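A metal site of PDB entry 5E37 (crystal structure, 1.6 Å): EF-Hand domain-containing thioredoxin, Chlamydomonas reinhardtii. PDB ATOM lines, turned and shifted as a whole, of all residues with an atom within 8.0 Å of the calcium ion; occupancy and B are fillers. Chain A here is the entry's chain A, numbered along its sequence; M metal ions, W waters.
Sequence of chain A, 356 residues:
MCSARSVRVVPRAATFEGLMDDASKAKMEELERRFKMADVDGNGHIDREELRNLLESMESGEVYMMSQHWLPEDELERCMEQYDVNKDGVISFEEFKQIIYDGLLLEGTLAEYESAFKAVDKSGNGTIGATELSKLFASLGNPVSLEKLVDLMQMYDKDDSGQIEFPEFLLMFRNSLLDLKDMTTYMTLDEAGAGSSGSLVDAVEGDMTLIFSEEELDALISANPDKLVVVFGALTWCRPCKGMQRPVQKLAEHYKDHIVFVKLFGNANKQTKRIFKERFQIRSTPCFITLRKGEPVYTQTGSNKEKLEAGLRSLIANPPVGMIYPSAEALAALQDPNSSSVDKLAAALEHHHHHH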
ATOM      1  N   HIS A  45     -17.789  22.217  33.581  1.00  0.00           N
ATOM      2  CA  HIS A  45     -17.994  23.137  32.430  1.00  0.00           C
ATOM      3  C   HIS A  45     -19.405  23.090  31.780  1.00  0.00           C
ATOM      4  O   HIS A  45     -20.151  22.207  32.118  1.00  0.00           O
ATOM      5  CB  HIS A  45     -16.896  22.938  31.397  1.00  0.00           C
ATOM      6  CG  HIS A  45     -16.986  21.652  30.640  1.00  0.00           C
ATOM      7  ND1 HIS A  45     -17.091  21.606  29.266  1.00  0.00           N
ATOM      8  CD2 HIS A  45     -16.916  20.370  31.059  1.00  0.00           C
ATOM      9  CE1 HIS A  45     -17.127  20.344  28.875  1.00  0.00           C
ATOM     10  NE2 HIS A  45     -17.029  19.574  29.944  1.00  0.00           N
ATOM     11  N   ILE A  46     -19.740  24.056  30.901  1.00  0.00           N
ATOM     12  CA  ILE A  46     -21.108  24.143  30.258  1.00  0.00           C
ATOM     13  C   ILE A  46     -21.099  23.683  28.792  1.00  0.00           C
ATOM     14  O   ILE A  46     -20.713  24.404  27.853  1.00  0.00           O
ATOM     15  CB  ILE A  46     -21.710  25.578  30.373  1.00  0.00           C
ATOM     16  CG1 ILE A  46     -21.854  25.966  31.842  1.00  0.00           C
ATOM     17  CG2 ILE A  46     -23.044  25.685  29.622  1.00  0.00           C
ATOM     18  CD1 ILE A  46     -22.203  27.439  31.977  1.00  0.00           C
ATOM     19  N   MET A  80     -23.171  29.883  20.545  1.00  0.00           N
ATOM     20  CA  MET A  80     -21.825  29.221  20.679  1.00  0.00           C
ATOM     21  C   MET A  80     -20.812  29.938  19.775  1.00  0.00           C
ATOM     22  O   MET A  80     -19.676  30.098  20.176  1.00  0.00           O
ATOM     23  CB  MET A  80     -21.852  27.723  20.276  1.00  0.00           C
ATOM     24  CG  MET A  80     -22.340  26.730  21.341  1.00  0.00           C
ATOM     25  SD  MET A  80     -21.491  26.621  22.918  1.00  0.00           S
ATOM     26  CE  MET A  80     -19.781  26.411  22.525  1.00  0.00           C
ATOM     27  N   TYR A  83     -19.618  33.199  21.880  1.00  0.00           N
ATOM     28  CA  TYR A  83     -19.003  33.144  23.236  1.00  0.00           C
ATOM     29  C   TYR A  83     -17.977  32.089  23.455  1.00  0.00           C
ATOM     30  O   TYR A  83     -17.266  32.150  24.464  1.00  0.00           O
ATOM     31  CB  TYR A  83     -20.087  33.101  24.336  1.00  0.00           C
ATOM     32  CG  TYR A  83     -20.905  34.351  24.260  1.00  0.00           C
ATOM     33  CD1 TYR A  83     -20.433  35.531  24.816  1.00  0.00           C
ATOM     34  CD2 TYR A  83     -22.113  34.386  23.556  1.00  0.00           C
ATOM     35  CE1 TYR A  83     -21.157  36.716  24.701  1.00  0.00           C
ATOM     36  CE2 TYR A  83     -22.845  35.560  23.441  1.00  0.00           C
ATOM     37  CZ  TYR A  83     -22.343  36.722  24.018  1.00  0.00           C
ATOM     38  OH  TYR A  83     -23.031  37.884  23.907  1.00  0.00           O
ATOM     39  N   ASP A  84     -17.908  31.119  22.533  1.00  0.00           N
ATOM     40  CA  ASP A  84     -16.868  30.064  22.524  1.00  0.00           C
ATOM     41  C   ASP A  84     -15.649  30.602  21.736  1.00  0.00           C
ATOM     42  O   ASP A  84     -15.552  30.391  20.516  1.00  0.00           O
ATOM     43  CB  ASP A  84     -17.464  28.797  21.865  1.00  0.00           C
ATOM     44  CG  ASP A  84     -16.510  27.579  21.862  1.00  0.00           C
ATOM     45  OD1 ASP A  84     -16.612  26.767  20.874  1.00  0.00           O
ATOM     46  OD2 ASP A  84     -15.732  27.405  22.839  1.00  0.00           O
ATOM     47  N   VAL A  85     -14.743  31.317  22.410  1.00  0.00           N
ATOM     48  CA  VAL A  85     -13.732  32.134  21.703  1.00  0.00           C
ATOM     49  C   VAL A  85     -12.544  31.282  21.277  1.00  0.00           C
ATOM     50  O   VAL A  85     -11.997  31.496  20.192  1.00  0.00           O
ATOM     51  CB  VAL A  85     -13.292  33.380  22.526  1.00  0.00           C
ATOM     52  CG1 VAL A  85     -12.297  34.227  21.730  1.00  0.00           C
ATOM     53  CG2 VAL A  85     -14.506  34.246  22.915  1.00  0.00           C
ATOM     54  N   ASN A  86     -12.137  30.325  22.118  1.00  0.00           N
ATOM     55  CA  ASN A  86     -11.087  29.374  21.751  1.00  0.00           C
ATOM     56  C   ASN A  86     -11.549  28.221  20.839  1.00  0.00           C
ATOM     57  O   ASN A  86     -10.730  27.501  20.271  1.00  0.00           O
ATOM     58  CB  ASN A  86     -10.423  28.812  23.008  1.00  0.00           C
ATOM     59  CG  ASN A  86     -11.408  28.198  23.942  1.00  0.00           C
ATOM     60  OD1 ASN A  86     -12.600  28.290  23.703  1.00  0.00           O
ATOM     61  ND2 ASN A  86     -10.935  27.596  25.006  1.00  0.00           N
ATOM     62  N   LYS A  87     -12.865  28.037  20.701  1.00  0.00           N
ATOM     63  CA  LYS A  87     -13.434  27.079  19.732  1.00  0.00           C
ATOM     64  C   LYS A  87     -13.244  25.586  20.117  1.00  0.00           C
ATOM     65  O   LYS A  87     -13.024  24.749  19.237  1.00  0.00           O
ATOM     66  CB  LYS A  87     -12.943  27.381  18.311  1.00  0.00           C
ATOM     67  N   ASP A  88     -13.353  25.259  21.409  1.00  0.00           N
ATOM     68  CA  ASP A  88     -13.351  23.866  21.901  1.00  0.00           C
ATOM     69  C   ASP A  88     -14.786  23.273  22.173  1.00  0.00           C
ATOM     70  O   ASP A  88     -14.952  22.392  23.045  1.00  0.00           O
ATOM     71  CB  ASP A  88     -12.510  23.757  23.174  1.00  0.00           C
ATOM     72  CG  ASP A  88     -13.172  24.377  24.390  1.00  0.00           C
ATOM     73  OD1 ASP A  88     -14.022  25.292  24.216  1.00  0.00           O
ATOM     74  OD2 ASP A  88     -12.856  23.925  25.506  1.00  0.00           O
ATOM     75  N   GLY A  89     -15.784  23.761  21.427  1.00  0.00           N
ATOM     76  CA  GLY A  89     -17.212  23.384  21.591  1.00  0.00           C
ATOM     77  C   GLY A  89     -17.867  23.418  22.979  1.00  0.00           C
ATOM     78  O   GLY A  89     -18.936  22.847  23.172  1.00  0.00           O
ATOM     79  N   VAL A  90     -17.245  24.070  23.957  1.00  0.00           N
ATOM     80  CA  VAL A  90     -17.823  24.122  25.264  1.00  0.00           C
ATOM     81  C   VAL A  90     -17.625  25.507  25.897  1.00  0.00           C
ATOM     82  O   VAL A  90     -16.730  26.228  25.506  1.00  0.00           O
ATOM     83  CB  VAL A  90     -17.244  23.047  26.168  1.00  0.00           C
ATOM     84  CG1 VAL A  90     -17.597  21.653  25.627  1.00  0.00           C
ATOM     85  CG2 VAL A  90     -15.743  23.213  26.351  1.00  0.00           C
ATOM     86  N   ILE A  91     -18.473  25.858  26.872  1.00  0.00           N
ATOM     87  CA  ILE A  91     -18.370  27.171  27.519  1.00  0.00           C
ATOM     88  C   ILE A  91     -17.677  27.055  28.861  1.00  0.00           C
ATOM     89  O   ILE A  91     -18.143  26.429  29.817  1.00  0.00           O
ATOM     90  CB  ILE A  91     -19.760  27.824  27.707  1.00  0.00           C
ATOM     91  CG1 ILE A  91     -20.411  28.167  26.358  1.00  0.00           C
ATOM     92  CG2 ILE A  91     -19.670  29.046  28.626  1.00  0.00           C
ATOM     93  CD1 ILE A  91     -19.773  29.315  25.642  1.00  0.00           C
ATOM     94  N   SER A  92     -16.540  27.753  28.967  1.00  0.00           N
ATOM     95  CA  SER A  92     -15.785  27.802  30.212  1.00  0.00           C
ATOM     96  C   SER A  92     -16.360  28.873  31.072  1.00  0.00           C
ATOM     97  O   SER A  92     -17.119  29.715  30.590  1.00  0.00           O
ATOM     98  CB  SER A  92     -14.312  28.192  29.953  1.00  0.00           C
ATOM     99  OG  SER A  92     -14.276  29.407  29.222  1.00  0.00           O
ATOM    100  N   GLU A  95     -15.792  32.284  29.616  1.00  0.00           N
ATOM    101  CA  GLU A  95     -16.661  32.559  28.507  1.00  0.00           C
ATOM    102  C   GLU A  95     -18.089  32.828  29.015  1.00  0.00           C
ATOM    103  O   GLU A  95     -18.830  33.622  28.402  1.00  0.00           O
ATOM    104  CB  GLU A  95     -16.603  31.364  27.563  1.00  0.00           C
ATOM    105  CG  GLU A  95     -15.218  31.223  26.892  1.00  0.00           C
ATOM    106  CD  GLU A  95     -15.179  30.104  25.872  1.00  0.00           C
ATOM    107  OE1 GLU A  95     -14.654  30.314  24.762  1.00  0.00           O
ATOM    108  OE2 GLU A  95     -15.687  29.001  26.178  1.00  0.00           O
HETATM  109 CA    CA M   1     -14.896  27.451  24.437  1.00  0.00          CA
HETATM  110  O   HOH W   1     -14.254  26.800  26.019  1.00  0.00           O
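The backbone NH (N) of Glu 95 sits close to the side-chain hydroxyl (OG) of Ser 92 (3.3 Å).
N of Gly 89 sits at hydrogen-bond distance from OD1 of Asp 84.
The backbone NH (N) of Val 85 sits close to the side-chain carboxylate (OE1) of Glu 95 (2.6 Å).
Within 4 Å of the calcium ion: Asp 84, Asn 86, Asp 88, Val 90 and Glu 95.
The calcium ion is bound by OD2 of Asp 84, at 1.8 Å.
The calcium ion is bound by water W1 (1.8 Å).
The calcium ion is bound by the side-chain carboxylate (OD1) of Asp 88 (2.3 Å).
The backbone carbonyl oxygen (O) of Val 90 is bound to the calcium ion, 2.4 Å away.
OE2 of Glu 95 binds the calcium ion, at 2.5 Å.
The side-chain amide oxygen (OD1) of Asn 86 binds the calcium ion, 2.6 Å away.
OE1 of Glu 95 is bound to the calcium ion, 2.9 Å away.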
